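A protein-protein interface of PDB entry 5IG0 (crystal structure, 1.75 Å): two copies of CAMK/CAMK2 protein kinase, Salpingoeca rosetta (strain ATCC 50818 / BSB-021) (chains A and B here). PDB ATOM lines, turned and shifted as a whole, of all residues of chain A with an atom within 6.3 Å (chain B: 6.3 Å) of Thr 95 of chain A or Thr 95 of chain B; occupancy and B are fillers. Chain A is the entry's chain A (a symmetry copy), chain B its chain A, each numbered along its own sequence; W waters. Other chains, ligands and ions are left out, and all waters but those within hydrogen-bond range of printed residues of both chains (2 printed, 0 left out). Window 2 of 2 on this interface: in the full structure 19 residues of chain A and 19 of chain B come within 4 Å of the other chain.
OG1 of Thr 95 of chain A is in hydrogen-bond range of OG1 of Thr 95 of chain B (2.9 Å).
The backbone carbonyl oxygen of Gln 90 of chain A is in hydrogen-bond range of the backbone NH of Ile 97 of chain A, at 2.9 Å. The backbone carbonyl oxygen (O) of Gln 90 of chain B sits at hydrogen-bond distance from the backbone NH (N) of Ile 97 of chain B, at 2.9 Å.
Among the printed residues, merely in contact across the chains: Ile 97 of chain A with Val 122 of chain B (3.8 Å) and Val 122 of chain A with Ile 97 of chain B (3.8 Å).
Gly 93 of chain A touches none of the printed residues of chain B. Thr 95 of chain A touches just one residue of chain B: Thr 95. Of the printed residues of chain B, Ile 97 of chain A touches Val 122 (3.8 Å). Of the printed residues of chain B, Val 122 of chain A touches Ile 97. Met 91 of chain B touches none of the printed residues of chain A. Thr 95 of chain B touches one residue of chain A. Of the printed residues of chain A, Ile 97 of chain B touches Val 122 (3.8 Å). Of the printed residues of chain A, Val 122 of chain B touches Ile 97 (3.8 Å). The nearest residue of chain A that does not touch Thr 95 of chain B is Phe 92 of chain A (4.1 Å). The nearest printed residue of chain B that does not touch Ile 97 of chain A is Val 124 of chain B (6.1 Å).
Printed residues of chain B that touch a printed residue of chain A: Thr 95, Ile 97 and Val 122. Hydrophobic or aromatic side chains of chain B that line the printed part of chain A: Ile 97 and Val 122. Hydrophobic or aromatic side chains of chain A within 4 Å of the printed part of chain B: Ile 97 and Val 122. Among the printed residues, no Asp or Glu carboxylate lies within 4 Å of a Lys or Arg side-chain nitrogen of the other chain.
Thr 95 of chain B touches its own counterpart, Thr 95 of chain A. Ile 97 of chain A touches Val 122 of chain B, and with the chains exchanged Val 122 of chain A touches Ile 97 of chain B. Positions printed for both chains: 90, 91, 92, 93, 94, 95, 96, 97, 122, 123, 124, 125 and 133. Of the 3 pairs that touch across the chains among the printed residues, 3 have their exchanged pair printed and touching as well.
Water W2 lies within hydrogen-bond range of OG1 of Thr 95 of chain B (2.6 Å) and O of Phe 92 of chain A (2.7 Å). Water W1 bridges the side-chain hydroxyl (OG1) of Thr 95 of chain A and the backbone carbonyl oxygen (O) of Phe 92 of chain B.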
ATOM      1  N   GLN A  90     -22.253 -15.028 -30.752  1.00  0.00           N
ATOM      2  CA  GLN A  90     -22.676 -14.737 -29.397  1.00  0.00           C
ATOM      3  C   GLN A  90     -22.992 -16.044 -28.700  1.00  0.00           C
ATOM      4  O   GLN A  90     -23.734 -16.870 -29.227  1.00  0.00           O
ATOM      5  CB  GLN A  90     -23.894 -13.818 -29.403  1.00  0.00           C
ATOM      6  CG  GLN A  90     -23.674 -12.529 -30.177  1.00  0.00           C
ATOM      7  CD  GLN A  90     -24.963 -11.771 -30.441  1.00  0.00           C
ATOM      8  OE1 GLN A  90     -25.543 -11.862 -31.535  1.00  0.00           O
ATOM      9  NE2 GLN A  90     -25.442 -11.054 -29.426  1.00  0.00           N
ATOM     10  N   MET A  91     -22.405 -16.228 -27.521  1.00  0.00           N
ATOM     11  CA  MET A  91     -22.532 -17.469 -26.768  1.00  0.00           C
ATOM     12  C   MET A  91     -23.568 -17.341 -25.668  1.00  0.00           C
ATOM     13  O   MET A  91     -23.571 -16.362 -24.921  1.00  0.00           O
ATOM     14  CB  MET A  91     -21.189 -17.858 -26.145  1.00  0.00           C
ATOM     15  CG  MET A  91     -20.040 -17.944 -27.125  1.00  0.00           C
ATOM     16  SD  MET A  91     -20.292 -19.201 -28.391  1.00  0.00           S
ATOM     17  CE  MET A  91     -20.384 -20.676 -27.387  1.00  0.00           C
ATOM     18  N   PHE A  92     -24.436 -18.340 -25.571  1.00  0.00           N
ATOM     19  CA  PHE A  92     -25.410 -18.430 -24.492  1.00  0.00           C
ATOM     20  C   PHE A  92     -25.428 -19.865 -23.993  1.00  0.00           C
ATOM     21  O   PHE A  92     -26.168 -20.705 -24.498  1.00  0.00           O
ATOM     22  CB  PHE A  92     -26.794 -17.983 -24.968  1.00  0.00           C
ATOM     23  CG  PHE A  92     -26.807 -16.591 -25.531  1.00  0.00           C
ATOM     24  CD1 PHE A  92     -27.003 -15.497 -24.706  1.00  0.00           C
ATOM     25  CD2 PHE A  92     -26.593 -16.376 -26.880  1.00  0.00           C
ATOM     26  CE1 PHE A  92     -27.000 -14.214 -25.224  1.00  0.00           C
ATOM     27  CE2 PHE A  92     -26.589 -15.096 -27.400  1.00  0.00           C
ATOM     28  CZ  PHE A  92     -26.791 -14.016 -26.570  1.00  0.00           C
ATOM     29  N   GLY A  93     -24.583 -20.147 -23.010  1.00  0.00           N
ATOM     30  CA  GLY A  93     -24.419 -21.506 -22.533  1.00  0.00           C
ATOM     31  C   GLY A  93     -23.891 -22.388 -23.647  1.00  0.00           C
ATOM     32  O   GLY A  93     -22.841 -22.104 -24.228  1.00  0.00           O
ATOM     33  N   ASP A  94     -24.629 -23.452 -23.955  1.00  0.00           N
ATOM     34  CA  ASP A  94     -24.226 -24.396 -24.989  1.00  0.00           C
ATOM     35  C   ASP A  94     -24.730 -23.975 -26.366  1.00  0.00           C
ATOM     36  O   ASP A  94     -24.588 -24.725 -27.329  1.00  0.00           O
ATOM     37  CB  ASP A  94     -24.743 -25.798 -24.665  1.00  0.00           C
ATOM     38  CG  ASP A  94     -24.049 -26.416 -23.463  1.00  0.00           C
ATOM     39  OD1 ASP A  94     -22.925 -25.979 -23.128  1.00  0.00           O
ATOM     40  OD2 ASP A  94     -24.626 -27.344 -22.857  1.00  0.00           O
ATOM     41  N   THR A  95     -25.315 -22.783 -26.449  1.00  0.00           N
ATOM     42  CA  THR A  95     -25.823 -22.258 -27.717  1.00  0.00           C
ATOM     43  C   THR A  95     -24.904 -21.172 -28.262  1.00  0.00           C
ATOM     44  O   THR A  95     -24.433 -20.316 -27.517  1.00  0.00           O
ATOM     45  CB  THR A  95     -27.242 -21.683 -27.559  1.00  0.00           C
ATOM     46  OG1 THR A  95     -28.139 -22.730 -27.176  1.00  0.00           O
ATOM     47  CG2 THR A  95     -27.734 -21.073 -28.870  1.00  0.00           C
ATOM     48  N   ALA A  96     -24.654 -21.225 -29.569  1.00  0.00           N
ATOM     49  CA  ALA A  96     -23.889 -20.197 -30.261  1.00  0.00           C
ATOM     50  C   ALA A  96     -24.716 -19.626 -31.408  1.00  0.00           C
ATOM     51  O   ALA A  96     -25.197 -20.370 -32.259  1.00  0.00           O
ATOM     52  CB  ALA A  96     -22.576 -20.762 -30.785  1.00  0.00           C
ATOM     53  N   ILE A  97     -24.887 -18.310 -31.415  1.00  0.00           N
ATOM     54  CA  ILE A  97     -25.595 -17.638 -32.500  1.00  0.00           C
ATOM     55  C   ILE A  97     -24.567 -16.995 -33.410  1.00  0.00           C
ATOM     56  O   ILE A  97     -23.905 -16.040 -33.016  1.00  0.00           O
ATOM     57  CB  ILE A  97     -26.574 -16.567 -31.981  1.00  0.00           C
ATOM     58  CG1 ILE A  97     -27.557 -17.180 -30.977  1.00  0.00           C
ATOM     59  CG2 ILE A  97     -27.334 -15.935 -33.146  1.00  0.00           C
ATOM     60  CD1 ILE A  97     -28.410 -16.161 -30.268  1.00  0.00           C
ATOM     61  N   VAL A 122     -27.844 -20.983 -35.822  1.00  0.00           N
ATOM     62  CA  VAL A 122     -27.866 -21.363 -34.410  1.00  0.00           C
ATOM     63  C   VAL A 122     -27.222 -22.729 -34.238  1.00  0.00           C
ATOM     64  O   VAL A 122     -27.745 -23.737 -34.717  1.00  0.00           O
ATOM     65  CB  VAL A 122     -29.294 -21.406 -33.835  1.00  0.00           C
ATOM     66  CG1 VAL A 122     -29.245 -21.624 -32.321  1.00  0.00           C
ATOM     67  CG2 VAL A 122     -30.039 -20.121 -34.159  1.00  0.00           C
ATOM     68  N   TRP A 123     -26.088 -22.741 -33.548  1.00  0.00           N
ATOM     69  CA  TRP A 123     -25.314 -23.955 -33.315  1.00  0.00           C
ATOM     70  C   TRP A 123     -25.428 -24.361 -31.853  1.00  0.00           C
ATOM     71  O   TRP A 123     -25.515 -23.502 -30.976  1.00  0.00           O
ATOM     72  CB  TRP A 123     -23.844 -23.742 -33.669  1.00  0.00           C
ATOM     73  CG  TRP A 123     -23.568 -23.504 -35.121  1.00  0.00           C
ATOM     74  CD1 TRP A 123     -23.626 -22.313 -35.785  1.00  0.00           C
ATOM     75  CD2 TRP A 123     -23.162 -24.481 -36.085  1.00  0.00           C
ATOM     76  NE1 TRP A 123     -23.290 -22.490 -37.109  1.00  0.00           N
ATOM     77  CE2 TRP A 123     -22.998 -23.816 -37.317  1.00  0.00           C
ATOM     78  CE3 TRP A 123     -22.924 -25.859 -36.028  1.00  0.00           C
ATOM     79  CZ2 TRP A 123     -22.611 -24.481 -38.481  1.00  0.00           C
ATOM     80  CZ3 TRP A 123     -22.539 -26.517 -37.182  1.00  0.00           C
ATOM     81  CH2 TRP A 123     -22.385 -25.828 -38.392  1.00  0.00           C
ATOM     82  N   VAL A 124     -25.406 -25.666 -31.600  1.00  0.00           N
ATOM     83  CA  VAL A 124     -25.501 -26.184 -30.240  1.00  0.00           C
ATOM     84  C   VAL A 124     -24.370 -27.173 -29.994  1.00  0.00           C
ATOM     85  O   VAL A 124     -24.016 -27.948 -30.878  1.00  0.00           O
ATOM     86  CB  VAL A 124     -26.867 -26.854 -29.993  1.00  0.00           C
ATOM     87  CG1 VAL A 124     -26.923 -27.492 -28.616  1.00  0.00           C
ATOM     88  CG2 VAL A 124     -27.983 -25.826 -30.143  1.00  0.00           C
ATOM     89  N   LYS A 125     -23.789 -27.121 -28.799  1.00  0.00           N
ATOM     90  CA  LYS A 125     -22.719 -28.042 -28.434  1.00  0.00           C
ATOM     91  C   LYS A 125     -23.223 -29.472 -28.432  1.00  0.00           C
ATOM     92  O   LYS A 125     -24.314 -29.759 -27.934  1.00  0.00           O
ATOM     93  CB  LYS A 125     -22.151 -27.712 -27.053  1.00  0.00           C
ATOM     94  CG  LYS A 125     -21.225 -26.524 -27.021  1.00  0.00           C
ATOM     95  CD  LYS A 125     -20.589 -26.375 -25.648  1.00  0.00           C
ATOM     96  CE  LYS A 125     -19.901 -25.032 -25.500  1.00  0.00           C
ATOM     97  NZ  LYS A 125     -19.184 -24.922 -24.203  1.00  0.00           N
ATOM     98  N   TRP A 133     -20.055 -29.571 -32.460  1.00  0.00           N
ATOM     99  CA  TRP A 133     -21.153 -28.632 -32.665  1.00  0.00           C
ATOM    100  C   TRP A 133     -22.116 -29.152 -33.725  1.00  0.00           C
ATOM    101  O   TRP A 133     -21.700 -29.839 -34.656  1.00  0.00           O
ATOM    102  CB  TRP A 133     -20.618 -27.269 -33.095  1.00  0.00           C
ATOM    103  CG  TRP A 133     -19.838 -26.560 -32.047  1.00  0.00           C
ATOM    104  CD1 TRP A 133     -18.489 -26.609 -31.849  1.00  0.00           C
ATOM    105  CD2 TRP A 133     -20.361 -25.681 -31.047  1.00  0.00           C
ATOM    106  NE1 TRP A 133     -18.138 -25.812 -30.787  1.00  0.00           N
ATOM    107  CE2 TRP A 133     -19.270 -25.236 -30.273  1.00  0.00           C
ATOM    108  CE3 TRP A 133     -21.644 -25.225 -30.733  1.00  0.00           C
ATOM    109  CZ2 TRP A 133     -19.424 -24.355 -29.208  1.00  0.00           C
ATOM    110  CZ3 TRP A 133     -21.796 -24.354 -29.674  1.00  0.00           C
ATOM    111  CH2 TRP A 133     -20.692 -23.928 -28.924  1.00  0.00           C
ATOM    112  N   GLN B  90     -38.570 -24.524 -30.421  1.00  0.00           N
ATOM    113  CA  GLN B  90     -37.645 -25.621 -30.221  1.00  0.00           C
ATOM    114  C   GLN B  90     -36.731 -25.277 -29.063  1.00  0.00           C
ATOM    115  O   GLN B  90     -36.148 -24.196 -29.028  1.00  0.00           O
ATOM    116  CB  GLN B  90     -36.838 -25.879 -31.490  1.00  0.00           C
ATOM    117  CG  GLN B  90     -37.702 -26.131 -32.715  1.00  0.00           C
ATOM    118  CD  GLN B  90     -36.916 -26.079 -34.012  1.00  0.00           C
ATOM    119  OE1 GLN B  90     -36.916 -25.056 -34.716  1.00  0.00           O
ATOM    120  NE2 GLN B  90     -36.207 -27.165 -34.316  1.00  0.00           N
ATOM    121  N   MET B  91     -36.631 -26.199 -28.111  1.00  0.00           N
ATOM    122  CA  MET B  91     -35.868 -25.983 -26.889  1.00  0.00           C
ATOM    123  C   MET B  91     -34.504 -26.640 -26.969  1.00  0.00           C
ATOM    124  O   MET B  91     -34.389 -27.799 -27.369  1.00  0.00           O
ATOM    125  CB  MET B  91     -36.621 -26.545 -25.679  1.00  0.00           C
ATOM    126  CG  MET B  91     -38.035 -26.031 -25.522  1.00  0.00           C
ATOM    127  SD  MET B  91     -38.109 -24.249 -25.269  1.00  0.00           S
ATOM    128  CE  MET B  91     -37.200 -24.089 -23.739  1.00  0.00           C
ATOM    129  N   PHE B  92     -33.478 -25.895 -26.577  1.00  0.00           N
ATOM    130  CA  PHE B  92     -32.123 -26.418 -26.474  1.00  0.00           C
ATOM    131  C   PHE B  92     -31.525 -25.918 -25.170  1.00  0.00           C
ATOM    132  O   PHE B  92     -30.929 -24.846 -25.113  1.00  0.00           O
ATOM    133  CB  PHE B  92     -31.281 -25.993 -27.679  1.00  0.00           C
ATOM    134  CG  PHE B  92     -31.873 -26.411 -28.994  1.00  0.00           C
ATOM    135  CD1 PHE B  92     -31.586 -27.651 -29.535  1.00  0.00           C
ATOM    136  CD2 PHE B  92     -32.741 -25.574 -29.672  1.00  0.00           C
ATOM    137  CE1 PHE B  92     -32.143 -28.040 -30.740  1.00  0.00           C
ATOM    138  CE2 PHE B  92     -33.300 -25.960 -30.875  1.00  0.00           C
ATOM    139  CZ  PHE B  92     -33.001 -27.195 -31.407  1.00  0.00           C
ATOM    140  N   GLY B  93     -31.711 -26.696 -24.110  1.00  0.00           N
ATOM    141  CA  GLY B  93     -31.295 -26.270 -22.789  1.00  0.00           C
ATOM    142  C   GLY B  93     -32.052 -25.020 -22.384  1.00  0.00           C
ATOM    143  O   GLY B  93     -33.285 -25.009 -22.370  1.00  0.00           O
ATOM    144  N   ASP B  94     -31.311 -23.961 -22.066  1.00  0.00           N
ATOM    145  CA  ASP B  94     -31.909 -22.704 -21.636  1.00  0.00           C
ATOM    146  C   ASP B  94     -32.230 -21.797 -22.819  1.00  0.00           C
ATOM    147  O   ASP B  94     -32.619 -20.647 -22.626  1.00  0.00           O
ATOM    148  CB  ASP B  94     -30.976 -21.970 -20.671  1.00  0.00           C
ATOM    149  CG  ASP B  94     -30.851 -22.673 -19.329  1.00  0.00           C
ATOM    150  OD1 ASP B  94     -31.754 -23.465 -18.979  1.00  0.00           O
ATOM    151  OD2 ASP B  94     -29.851 -22.426 -18.622  1.00  0.00           O
ATOM    152  N   THR B  95     -32.062 -22.316 -24.033  1.00  0.00           N
ATOM    153  CA  THR B  95     -32.354 -21.553 -25.247  1.00  0.00           C
ATOM    154  C   THR B  95     -33.654 -22.025 -25.885  1.00  0.00           C
ATOM    155  O   THR B  95     -33.913 -23.224 -25.971  1.00  0.00           O
ATOM    156  CB  THR B  95     -31.215 -21.676 -26.275  1.00  0.00           C
ATOM    157  OG1 THR B  95     -30.019 -21.111 -25.730  1.00  0.00           O
ATOM    158  CG2 THR B  95     -31.562 -20.937 -27.566  1.00  0.00           C
ATOM    159  N   ALA B  96     -34.467 -21.066 -26.325  1.00  0.00           N
ATOM    160  CA  ALA B  96     -35.692 -21.355 -27.058  1.00  0.00           C
ATOM    161  C   ALA B  96     -35.667 -20.634 -28.402  1.00  0.00           C
ATOM    162  O   ALA B  96     -35.477 -19.421 -28.454  1.00  0.00           O
ATOM    163  CB  ALA B  96     -36.915 -20.935 -26.254  1.00  0.00           C
ATOM    164  N   ILE B  97     -35.846 -21.386 -29.481  1.00  0.00           N
ATOM    165  CA  ILE B  97     -35.917 -20.802 -30.816  1.00  0.00           C
ATOM    166  C   ILE B  97     -37.374 -20.756 -31.234  1.00  0.00           C
ATOM    167  O   ILE B  97     -37.983 -21.796 -31.465  1.00  0.00           O
ATOM    168  CB  ILE B  97     -35.104 -21.608 -31.847  1.00  0.00           C
ATOM    169  CG1 ILE B  97     -33.650 -21.754 -31.387  1.00  0.00           C
ATOM    170  CG2 ILE B  97     -35.159 -20.926 -33.214  1.00  0.00           C
ATOM    171  CD1 ILE B  97     -32.840 -22.701 -32.235  1.00  0.00           C
ATOM    172  N   VAL B 122     -34.753 -15.711 -30.860  1.00  0.00           N
ATOM    173  CA  VAL B 122     -33.979 -16.542 -29.939  1.00  0.00           C
ATOM    174  C   VAL B 122     -34.113 -15.998 -28.525  1.00  0.00           C
ATOM    175  O   VAL B 122     -33.648 -14.895 -28.228  1.00  0.00           O
ATOM    176  CB  VAL B 122     -32.487 -16.602 -30.313  1.00  0.00           C
ATOM    177  CG1 VAL B 122     -31.765 -17.626 -29.435  1.00  0.00           C
ATOM    178  CG2 VAL B 122     -32.320 -16.957 -31.782  1.00  0.00           C
ATOM    179  N   TRP B 123     -34.749 -16.789 -27.669  1.00  0.00           N
ATOM    180  CA  TRP B 123     -35.001 -16.415 -26.282  1.00  0.00           C
ATOM    181  C   TRP B 123     -34.119 -17.245 -25.361  1.00  0.00           C
ATOM    182  O   TRP B 123     -33.842 -18.409 -25.651  1.00  0.00           O
ATOM    183  CB  TRP B 123     -36.466 -16.635 -25.915  1.00  0.00           C
ATOM    184  CG  TRP B 123     -37.440 -15.749 -26.628  1.00  0.00           C
ATOM    185  CD1 TRP B 123     -37.992 -15.957 -27.859  1.00  0.00           C
ATOM    186  CD2 TRP B 123     -38.000 -14.525 -26.139  1.00  0.00           C
ATOM    187  NE1 TRP B 123     -38.856 -14.931 -28.172  1.00  0.00           N
ATOM    188  CE2 TRP B 123     -38.879 -14.039 -27.128  1.00  0.00           C
ATOM    189  CE3 TRP B 123     -37.839 -13.789 -24.960  1.00  0.00           C
ATOM    190  CZ2 TRP B 123     -39.591 -12.849 -26.975  1.00  0.00           C
ATOM    191  CZ3 TRP B 123     -38.547 -12.611 -24.809  1.00  0.00           C
ATOM    192  CH2 TRP B 123     -39.413 -12.152 -25.810  1.00  0.00           C
ATOM    193  N   VAL B 124     -33.701 -16.649 -24.249  1.00  0.00           N
ATOM    194  CA  VAL B 124     -32.855 -17.339 -23.281  1.00  0.00           C
ATOM    195  C   VAL B 124     -33.459 -17.199 -21.890  1.00  0.00           C
ATOM    196  O   VAL B 124     -33.986 -16.146 -21.542  1.00  0.00           O
ATOM    197  CB  VAL B 124     -31.417 -16.786 -23.303  1.00  0.00           C
ATOM    198  CG1 VAL B 124     -30.568 -17.424 -22.218  1.00  0.00           C
ATOM    199  CG2 VAL B 124     -30.790 -17.025 -24.671  1.00  0.00           C
ATOM    200  N   LYS B 125     -33.405 -18.275 -21.111  1.00  0.00           N
ATOM    201  CA  LYS B 125     -33.916 -18.251 -19.746  1.00  0.00           C
ATOM    202  C   LYS B 125     -33.140 -17.260 -18.901  1.00  0.00           C
ATOM    203  O   LYS B 125     -31.911 -17.197 -18.969  1.00  0.00           O
ATOM    204  CB  LYS B 125     -33.831 -19.633 -19.099  1.00  0.00           C
ATOM    205  CG  LYS B 125     -34.892 -20.606 -19.547  1.00  0.00           C
ATOM    206  CD  LYS B 125     -34.823 -21.889 -18.734  1.00  0.00           C
ATOM    207  CE  LYS B 125     -35.665 -22.984 -19.358  1.00  0.00           C
ATOM    208  NZ  LYS B 125     -35.691 -24.207 -18.512  1.00  0.00           N
ATOM    209  N   TRP B 133     -37.695 -14.928 -19.179  1.00  0.00           N
ATOM    210  CA  TRP B 133     -37.088 -15.076 -20.498  1.00  0.00           C
ATOM    211  C   TRP B 133     -36.641 -13.724 -21.040  1.00  0.00           C
ATOM    212  O   TRP B 133     -37.265 -12.704 -20.751  1.00  0.00           O
ATOM    213  CB  TRP B 133     -38.076 -15.711 -21.473  1.00  0.00           C
ATOM    214  CG  TRP B 133     -38.418 -17.123 -21.164  1.00  0.00           C
ATOM    215  CD1 TRP B 133     -39.459 -17.571 -20.403  1.00  0.00           C
ATOM    216  CD2 TRP B 133     -37.719 -18.286 -21.617  1.00  0.00           C
ATOM    217  NE1 TRP B 133     -39.452 -18.944 -20.356  1.00  0.00           N
ATOM    218  CE2 TRP B 133     -38.390 -19.407 -21.087  1.00  0.00           C
ATOM    219  CE3 TRP B 133     -36.594 -18.488 -22.420  1.00  0.00           C
ATOM    220  CZ2 TRP B 133     -37.974 -20.710 -21.339  1.00  0.00           C
ATOM    221  CZ3 TRP B 133     -36.180 -19.781 -22.666  1.00  0.00           C
ATOM    222  CH2 TRP B 133     -36.869 -20.876 -22.127  1.00  0.00           C
HETATM  223  O   HOH W   1     -28.236 -24.721 -25.475  1.00  0.00           O
HETATM  224  O   HOH W   2     -28.654 -21.162 -23.495  1.00  0.00           O
